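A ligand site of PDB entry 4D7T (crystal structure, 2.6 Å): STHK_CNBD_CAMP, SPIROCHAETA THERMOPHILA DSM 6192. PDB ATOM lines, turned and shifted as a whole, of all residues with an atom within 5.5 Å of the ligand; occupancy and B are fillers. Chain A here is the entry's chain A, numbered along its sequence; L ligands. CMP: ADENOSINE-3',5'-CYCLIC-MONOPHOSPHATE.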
ATOM      1  N   ILE A 104      10.144  14.330  37.236  1.00  0.00           N
ATOM      2  CA  ILE A 104      11.476  13.972  36.750  1.00  0.00           C
ATOM      3  C   ILE A 104      12.286  15.237  36.481  1.00  0.00           C
ATOM      4  O   ILE A 104      11.753  16.214  35.928  1.00  0.00           O
ATOM      5  CB  ILE A 104      11.390  13.123  35.459  1.00  0.00           C
ATOM      6  CG1 ILE A 104      10.737  11.768  35.749  1.00  0.00           C
ATOM      7  CG2 ILE A 104      12.769  12.929  34.854  1.00  0.00           C
ATOM      8  CD1 ILE A 104      10.628  10.863  34.525  1.00  0.00           C
ATOM      9  N   GLY A 110      17.295   8.071  37.531  1.00  0.00           N
ATOM     10  CA  GLY A 110      16.179   7.152  37.712  1.00  0.00           C
ATOM     11  C   GLY A 110      15.841   6.414  36.435  1.00  0.00           C
ATOM     12  O   GLY A 110      16.206   6.858  35.336  1.00  0.00           O
ATOM     13  N   ASP A 112      12.675   4.525  36.620  1.00  0.00           N
ATOM     14  CA  ASP A 112      11.241   4.350  36.834  1.00  0.00           C
ATOM     15  C   ASP A 112      10.451   4.969  35.680  1.00  0.00           C
ATOM     16  O   ASP A 112      10.816   6.059  35.199  1.00  0.00           O
ATOM     17  CB  ASP A 112      10.796   4.967  38.167  1.00  0.00           C
ATOM     18  CG  ASP A 112      11.290   4.195  39.370  1.00  0.00           C
ATOM     19  OD1 ASP A 112      11.714   3.026  39.207  1.00  0.00           O
ATOM     20  OD2 ASP A 112      11.263   4.755  40.485  1.00  0.00           O
ATOM     21  N   VAL A 123       6.591  18.136  29.411  1.00  0.00           N
ATOM     22  CA  VAL A 123       7.944  17.676  29.144  1.00  0.00           C
ATOM     23  C   VAL A 123       8.812  18.876  28.784  1.00  0.00           C
ATOM     24  O   VAL A 123       8.600  19.512  27.745  1.00  0.00           O
ATOM     25  CB  VAL A 123       7.992  16.619  28.008  1.00  0.00           C
ATOM     26  CG1 VAL A 123       9.434  16.249  27.663  1.00  0.00           C
ATOM     27  CG2 VAL A 123       7.206  15.386  28.415  1.00  0.00           C
ATOM     28  N   TYR A 132       8.679  20.364  25.059  1.00  0.00           N
ATOM     29  CA  TYR A 132       8.694  19.364  23.999  1.00  0.00           C
ATOM     30  C   TYR A 132       7.327  18.727  23.786  1.00  0.00           C
ATOM     31  O   TYR A 132       7.016  18.300  22.672  1.00  0.00           O
ATOM     32  CB  TYR A 132       9.750  18.300  24.301  1.00  0.00           C
ATOM     33  CG  TYR A 132      11.164  18.843  24.285  1.00  0.00           C
ATOM     34  CD1 TYR A 132      11.848  19.044  23.092  1.00  0.00           C
ATOM     35  CD2 TYR A 132      11.836  19.151  25.466  1.00  0.00           C
ATOM     36  CE1 TYR A 132      13.133  19.547  23.067  1.00  0.00           C
ATOM     37  CE2 TYR A 132      13.123  19.647  25.448  1.00  0.00           C
ATOM     38  CZ  TYR A 132      13.765  19.843  24.248  1.00  0.00           C
ATOM     39  OH  TYR A 132      15.050  20.347  24.223  1.00  0.00           O
ATOM     40  N   ALA A 133       6.527  18.666  24.846  1.00  0.00           N
ATOM     41  CA  ALA A 133       5.234  17.990  24.768  1.00  0.00           C
ATOM     42  C   ALA A 133       4.299  18.301  25.938  1.00  0.00           C
ATOM     43  O   ALA A 133       4.699  18.867  26.953  1.00  0.00           O
ATOM     44  CB  ALA A 133       5.437  16.473  24.673  1.00  0.00           C
ATOM     45  N   LEU A 135       1.737  15.629  27.871  1.00  0.00           N
ATOM     46  CA  LEU A 135       1.251  14.252  27.933  1.00  0.00           C
ATOM     47  C   LEU A 135       0.083  14.151  28.914  1.00  0.00           C
ATOM     48  O   LEU A 135       0.067  14.813  29.959  1.00  0.00           O
ATOM     49  CB  LEU A 135       2.382  13.306  28.334  1.00  0.00           C
ATOM     50  CG  LEU A 135       3.596  13.289  27.406  1.00  0.00           C
ATOM     51  CD1 LEU A 135       4.695  12.344  27.910  1.00  0.00           C
ATOM     52  CD2 LEU A 135       3.164  12.905  26.004  1.00  0.00           C
ATOM     53  N   PHE A 140       2.553   7.947  28.609  1.00  0.00           N
ATOM     54  CA  PHE A 140       3.540   7.613  29.629  1.00  0.00           C
ATOM     55  C   PHE A 140       4.887   8.267  29.341  1.00  0.00           C
ATOM     56  O   PHE A 140       5.137   8.755  28.232  1.00  0.00           O
ATOM     57  CB  PHE A 140       3.686   6.094  29.734  1.00  0.00           C
ATOM     58  CG  PHE A 140       4.368   5.455  28.570  1.00  0.00           C
ATOM     59  CD1 PHE A 140       3.662   5.157  27.409  1.00  0.00           C
ATOM     60  CD2 PHE A 140       5.727   5.153  28.621  1.00  0.00           C
ATOM     61  CE1 PHE A 140       4.306   4.569  26.315  1.00  0.00           C
ATOM     62  CE2 PHE A 140       6.360   4.576  27.543  1.00  0.00           C
ATOM     63  CZ  PHE A 140       5.662   4.277  26.394  1.00  0.00           C
ATOM     64  N   PHE A 141       5.755   8.285  30.351  1.00  0.00           N
ATOM     65  CA  PHE A 141       7.055   8.932  30.223  1.00  0.00           C
ATOM     66  C   PHE A 141       8.052   8.352  31.222  1.00  0.00           C
ATOM     67  O   PHE A 141       7.663   7.617  32.133  1.00  0.00           O
ATOM     68  CB  PHE A 141       6.916  10.446  30.421  1.00  0.00           C
ATOM     69  CG  PHE A 141       6.358  10.830  31.766  1.00  0.00           C
ATOM     70  CD1 PHE A 141       7.211  11.054  32.848  1.00  0.00           C
ATOM     71  CD2 PHE A 141       4.994  10.965  31.960  1.00  0.00           C
ATOM     72  CE1 PHE A 141       6.711  11.402  34.089  1.00  0.00           C
ATOM     73  CE2 PHE A 141       4.483  11.323  33.200  1.00  0.00           C
ATOM     74  CZ  PHE A 141       5.339  11.539  34.270  1.00  0.00           C
ATOM     75  N   GLY A 142       9.327   8.696  31.063  1.00  0.00           N
ATOM     76  CA  GLY A 142      10.372   8.122  31.884  1.00  0.00           C
ATOM     77  C   GLY A 142      10.859   6.794  31.319  1.00  0.00           C
ATOM     78  O   GLY A 142      11.592   6.066  31.991  1.00  0.00           O
ATOM     79  N   GLU A 143      10.446   6.483  30.104  1.00  0.00           N
ATOM     80  CA  GLU A 143      10.792   5.224  29.458  1.00  0.00           C
ATOM     81  C   GLU A 143      12.153   5.263  28.752  1.00  0.00           C
ATOM     82  O   GLU A 143      12.776   4.228  28.532  1.00  0.00           O
ATOM     83  CB  GLU A 143       9.703   4.839  28.446  1.00  0.00           C
ATOM     84  CG  GLU A 143       9.808   5.555  27.099  1.00  0.00           C
ATOM     85  CD  GLU A 143       9.560   7.052  27.170  1.00  0.00           C
ATOM     86  OE1 GLU A 143       9.070   7.546  28.204  1.00  0.00           O
ATOM     87  OE2 GLU A 143       9.855   7.763  26.180  1.00  0.00           O
ATOM     88  N   MET A 144      12.606   6.470  28.412  1.00  0.00           N
ATOM     89  CA  MET A 144      13.817   6.636  27.602  1.00  0.00           C
ATOM     90  C   MET A 144      15.126   6.363  28.367  1.00  0.00           C
ATOM     91  O   MET A 144      16.108   5.929  27.772  1.00  0.00           O
ATOM     92  CB  MET A 144      13.848   8.048  26.999  1.00  0.00           C
ATOM     93  CG  MET A 144      12.939   8.226  25.791  1.00  0.00           C
ATOM     94  SD  MET A 144      12.677   9.940  25.277  1.00  0.00           S
ATOM     95  CE  MET A 144      14.354  10.510  25.029  1.00  0.00           C
ATOM     96  N   ALA A 145      15.122   6.606  29.671  1.00  0.00           N
ATOM     97  CA  ALA A 145      16.330   6.428  30.481  1.00  0.00           C
ATOM     98  C   ALA A 145      16.846   4.989  30.477  1.00  0.00           C
ATOM     99  O   ALA A 145      18.040   4.762  30.694  1.00  0.00           O
ATOM    100  CB  ALA A 145      16.077   6.869  31.914  1.00  0.00           C
ATOM    101  N   LEU A 146      15.967   4.025  30.245  1.00  0.00           N
ATOM    102  CA  LEU A 146      16.370   2.624  30.255  1.00  0.00           C
ATOM    103  C   LEU A 146      16.634   2.086  28.848  1.00  0.00           C
ATOM    104  O   LEU A 146      17.673   1.462  28.606  1.00  0.00           O
ATOM    105  CB  LEU A 146      15.328   1.755  30.952  1.00  0.00           C
ATOM    106  CG  LEU A 146      15.811   0.326  31.218  1.00  0.00           C
ATOM    107  CD1 LEU A 146      17.022   0.337  32.136  1.00  0.00           C
ATOM    108  CD2 LEU A 146      14.713  -0.565  31.798  1.00  0.00           C
ATOM    109  N   PRO A 151      20.908   8.875  31.195  1.00  0.00           N
ATOM    110  CA  PRO A 151      20.215   9.620  32.251  1.00  0.00           C
ATOM    111  C   PRO A 151      18.903  10.226  31.745  1.00  0.00           C
ATOM    112  O   PRO A 151      18.660  10.171  30.543  1.00  0.00           O
ATOM    113  CB  PRO A 151      21.207  10.716  32.619  1.00  0.00           C
ATOM    114  CG  PRO A 151      22.544  10.173  32.229  1.00  0.00           C
ATOM    115  CD  PRO A 151      22.278   9.359  30.984  1.00  0.00           C
ATOM    116  N   ARG A 152      18.083  10.782  32.635  1.00  0.00           N
ATOM    117  CA  ARG A 152      16.843  11.410  32.212  1.00  0.00           C
ATOM    118  C   ARG A 152      17.118  12.513  31.198  1.00  0.00           C
ATOM    119  O   ARG A 152      17.880  13.442  31.456  1.00  0.00           O
ATOM    120  CB  ARG A 152      16.091  11.983  33.412  1.00  0.00           C
ATOM    121  CG  ARG A 152      15.713  10.955  34.479  1.00  0.00           C
ATOM    122  CD  ARG A 152      14.736   9.926  33.951  1.00  0.00           C
ATOM    123  NE  ARG A 152      13.974   9.277  35.023  1.00  0.00           N
ATOM    124  CZ  ARG A 152      13.166   8.240  34.840  1.00  0.00           C
ATOM    125  NH1 ARG A 152      13.011   7.707  33.637  1.00  0.00           N
ATOM    126  NH2 ARG A 152      12.514   7.728  35.866  1.00  0.00           N
ATOM    127  N   THR A 153      16.491  12.384  30.022  1.00  0.00           N
ATOM    128  CA  THR A 153      16.762  13.275  28.890  1.00  0.00           C
ATOM    129  C   THR A 153      16.033  14.622  28.989  1.00  0.00           C
ATOM    130  O   THR A 153      16.368  15.559  28.263  1.00  0.00           O
ATOM    131  CB  THR A 153      16.362  12.609  27.558  1.00  0.00           C
ATOM    132  OG1 THR A 153      14.960  12.318  27.567  1.00  0.00           O
ATOM    133  CG2 THR A 153      17.153  11.312  27.360  1.00  0.00           C
ATOM    134  N   ALA A 154      15.047  14.695  29.885  1.00  0.00           N
ATOM    135  CA  ALA A 154      14.222  15.886  30.002  1.00  0.00           C
ATOM    136  C   ALA A 154      13.553  16.007  31.374  1.00  0.00           C
ATOM    137  O   ALA A 154      13.445  15.020  32.115  1.00  0.00           O
ATOM    138  CB  ALA A 154      13.157  15.898  28.898  1.00  0.00           C
ATOM    139  N   THR A 155      13.099  17.215  31.683  1.00  0.00           N
ATOM    140  CA  THR A 155      12.379  17.481  32.925  1.00  0.00           C
ATOM    141  C   THR A 155      10.864  17.302  32.722  1.00  0.00           C
ATOM    142  O   THR A 155      10.312  17.757  31.715  1.00  0.00           O
ATOM    143  CB  THR A 155      12.665  18.911  33.446  1.00  0.00           C
ATOM    144  OG1 THR A 155      14.019  19.008  33.895  1.00  0.00           O
ATOM    145  CG2 THR A 155      11.705  19.285  34.586  1.00  0.00           C
ATOM    146  N   VAL A 156      10.196  16.620  33.650  1.00  0.00           N
ATOM    147  CA  VAL A 156       8.746  16.454  33.584  1.00  0.00           C
ATOM    148  C   VAL A 156       8.044  17.057  34.790  1.00  0.00           C
ATOM    149  O   VAL A 156       8.251  16.612  35.924  1.00  0.00           O
ATOM    150  CB  VAL A 156       8.338  14.972  33.472  1.00  0.00           C
ATOM    151  CG1 VAL A 156       6.846  14.848  33.203  1.00  0.00           C
ATOM    152  CG2 VAL A 156       9.113  14.282  32.364  1.00  0.00           C
ATOM    153  N   ARG A 192      11.843   8.473  18.331  1.00  0.00           N
ATOM    154  CA  ARG A 192      11.235   9.648  17.702  1.00  0.00           C
ATOM    155  C   ARG A 192      11.230  10.836  18.649  1.00  0.00           C
ATOM    156  O   ARG A 192      11.195  11.991  18.218  1.00  0.00           O
ATOM    157  CB  ARG A 192       9.803   9.330  17.253  1.00  0.00           C
ATOM    158  CG  ARG A 192       9.291  10.212  16.106  1.00  0.00           C
ATOM    159  CD  ARG A 192       8.116   9.547  15.401  1.00  0.00           C
ATOM    160  NE  ARG A 192       8.379   8.118  15.203  1.00  0.00           N
ATOM    161  CZ  ARG A 192       7.569   7.266  14.583  1.00  0.00           C
ATOM    162  NH1 ARG A 192       6.419   7.683  14.076  1.00  0.00           N
ATOM    163  NH2 ARG A 192       7.919   5.988  14.471  1.00  0.00           N
ATOM    164  N   ARG A 193      11.272  10.548  19.949  1.00  0.00           N
ATOM    165  CA  ARG A 193      11.411  11.578  20.968  1.00  0.00           C
ATOM    166  C   ARG A 193      12.856  12.019  21.089  1.00  0.00           C
ATOM    167  O   ARG A 193      13.126  13.198  21.280  1.00  0.00           O
ATOM    168  CB  ARG A 193      10.899  11.056  22.315  1.00  0.00           C
ATOM    169  CG  ARG A 193       9.397  10.854  22.376  1.00  0.00           C
ATOM    170  CD  ARG A 193       9.004  10.226  23.690  1.00  0.00           C
ATOM    171  NE  ARG A 193       7.561  10.243  23.894  1.00  0.00           N
ATOM    172  CZ  ARG A 193       6.958   9.789  24.988  1.00  0.00           C
ATOM    173  NH1 ARG A 193       7.684   9.287  25.985  1.00  0.00           N
ATOM    174  NH2 ARG A 193       5.641   9.841  25.103  1.00  0.00           N
ATOM    175  N   GLU A 196      13.381  14.319  18.014  1.00  0.00           N
ATOM    176  CA  GLU A 196      12.791  15.639  18.151  1.00  0.00           C
ATOM    177  C   GLU A 196      13.277  16.346  19.426  1.00  0.00           C
ATOM    178  O   GLU A 196      12.550  17.159  20.012  1.00  0.00           O
ATOM    179  CB  GLU A 196      11.249  15.538  18.138  1.00  0.00           C
ATOM    180  CG  GLU A 196      10.640  14.874  19.381  1.00  0.00           C
ATOM    181  CD  GLU A 196       9.126  14.732  19.298  1.00  0.00           C
ATOM    182  OE1 GLU A 196       8.504  15.299  18.377  1.00  0.00           O
ATOM    183  OE2 GLU A 196       8.541  14.069  20.194  1.00  0.00           O
ATOM    184  N   LEU A 197      14.499  16.051  19.835  1.00  0.00           N
ATOM    185  CA  LEU A 197      15.045  16.543  21.095  1.00  0.00           C
ATOM    186  C   LEU A 197      16.404  17.198  20.882  1.00  0.00           C
ATOM    187  O   LEU A 197      16.917  17.874  21.773  1.00  0.00           O
ATOM    188  CB  LEU A 197      15.143  15.394  22.103  1.00  0.00           C
ATOM    189  CG  LEU A 197      15.043  15.674  23.601  1.00  0.00           C
ATOM    190  CD1 LEU A 197      13.616  16.069  23.940  1.00  0.00           C
ATOM    191  CD2 LEU A 197      15.442  14.440  24.393  1.00  0.00           C
HETATM  192  P   CMP L   1      13.392   9.693  30.446  1.00  0.00           P
HETATM  193  O1P CMP L   1      14.683   9.933  29.727  1.00  0.00           O
HETATM  194  O2P CMP L   1      13.483   8.375  31.292  1.00  0.00           O
HETATM  195  O5' CMP L   1      12.920  11.013  31.307  1.00  0.00           O
HETATM  196  C5' CMP L   1      12.412  12.213  30.785  1.00  0.00           C
HETATM  197  C4' CMP L   1      11.334  11.783  29.813  1.00  0.00           C
HETATM  198  O4' CMP L   1      10.803  12.827  29.057  1.00  0.00           O
HETATM  199  C3' CMP L   1      11.731  10.729  28.782  1.00  0.00           C
HETATM  200  O3' CMP L   1      12.130   9.536  29.420  1.00  0.00           O
HETATM  201  C2' CMP L   1      10.463  10.678  27.927  1.00  0.00           C
HETATM  202  O2' CMP L   1       9.474   9.920  28.520  1.00  0.00           O
HETATM  203  C1' CMP L   1       9.952  12.161  28.073  1.00  0.00           C
HETATM  204  N9  CMP L   1      10.290  12.851  26.815  1.00  0.00           N
HETATM  205  C8  CMP L   1      11.540  13.260  26.413  1.00  0.00           C
HETATM  206  N7  CMP L   1      11.476  13.854  25.222  1.00  0.00           N
HETATM  207  C5  CMP L   1      10.113  13.808  24.850  1.00  0.00           C
HETATM  208  C6  CMP L   1       9.375  14.260  23.706  1.00  0.00           C
HETATM  209  N6  CMP L   1       9.953  14.884  22.644  1.00  0.00           N
HETATM  210  N1  CMP L   1       8.024  14.055  23.659  1.00  0.00           N
HETATM  211  C2  CMP L   1       7.417  13.430  24.713  1.00  0.00           C
HETATM  212  N3  CMP L   1       7.985  12.956  25.850  1.00  0.00           N
HETATM  213  C4  CMP L   1       9.337  13.160  25.880  1.00  0.00           C
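OE1 of Glu 143 sits at hydrogen-bond distance from O2' of the ligand (2.4 Å).
An oxygen (O2P) of the ligand lies within salt-bridge range of the guanidinium group (NH1) of Arg 152, at 2.5 Å.
The backbone NH (N) of Gly 142 is in hydrogen-bond range of an oxygen (O2') of the ligand.
O2P of the ligand sits close to O of Gly 142 (3.1 Å).
N of Ala 145 sits at hydrogen-bond distance from O2P of the ligand, 2.9 Å away.
The side-chain carboxylate of Glu 196 sits at hydrogen-bond distance from a nitrogen (N6) of the ligand.
The backbone NH (N) of Thr 153 lies within hydrogen-bond range of an oxygen (O1P) of the ligand, at 3.1 Å.
O1P of the ligand is in hydrogen-bond range of OG1 of Thr 153 (3.2 Å).
An oxygen (O2') of the ligand sits at hydrogen-bond distance from the guanidinium group (NH1) of Arg 193 (3.2 Å).
The backbone NH (N) of Met 144 lies within hydrogen-bond range of an oxygen (O3') of the ligand, 3.3 Å away.
OE2 of Glu 143 lies within salt-bridge range of NH1 of Arg 193, at 2.7 Å.
The guanidinium group (NH1) of Arg 152 is in hydrogen-bond range of the backbone carbonyl oxygen (O) of Gly 142 (2.7 Å).
NE of Arg 152 lies within hydrogen-bond range of O of Gly 110.
The backbone carbonyl oxygen (O) of Asp 112 is in hydrogen-bond range of the guanidinium group (NH2) of Arg 152 (2.5 Å).
NH2 of Arg 193 lies within hydrogen-bond range of O of Phe 140, 3.4 Å away.
O of Ala 133 sits at hydrogen-bond distance from N of Val 123, at 3.2 Å.
The backbone NH (N) of Tyr 132 lies within hydrogen-bond range of the backbone carbonyl oxygen (O) of Val 123.
The backbone carbonyl oxygen (O) of Ile 104 is in hydrogen-bond range of the backbone NH (N) of Val 156, at 2.8 Å.
CD1 of Ile 104 touches O5' of the ligand (3.95 Å).
Val 123 touches the ligand (CG1 to C4, 3.6 Å).
Tyr 132 touches the ligand (CB to N6, 3.8 Å).
Ala 133 touches the ligand (CB to C2, 3.6 Å).
CD1 of Leu 135 touches N3 of the ligand, at 3.9 Å.
Phe 141 touches the ligand (CA to O2', 3.1 Å).
O of Ala 154 touches C5' of the ligand (3.3 Å).
Val 156 touches the ligand.
CD1 of Leu 197 touches N7 of the ligand, at 3.3 Å.
Hydrophobic or aromatic side chains that line the ligand: Ile 104, Val 123, Tyr 132, Ala 133, Leu 135, Phe 141, Met 144, Ala 145, Ala 154, Val 156 and Leu 197.
17 residues have an atom within 4 Å of the ligand: Ile 104, Val 123, Tyr 132, Ala 133, Leu 135, Phe 141, Gly 142, Glu 143, Met 144, Ala 145, Arg 152, Thr 153, Ala 154, Val 156, Arg 193, Glu 196 and Leu 197.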
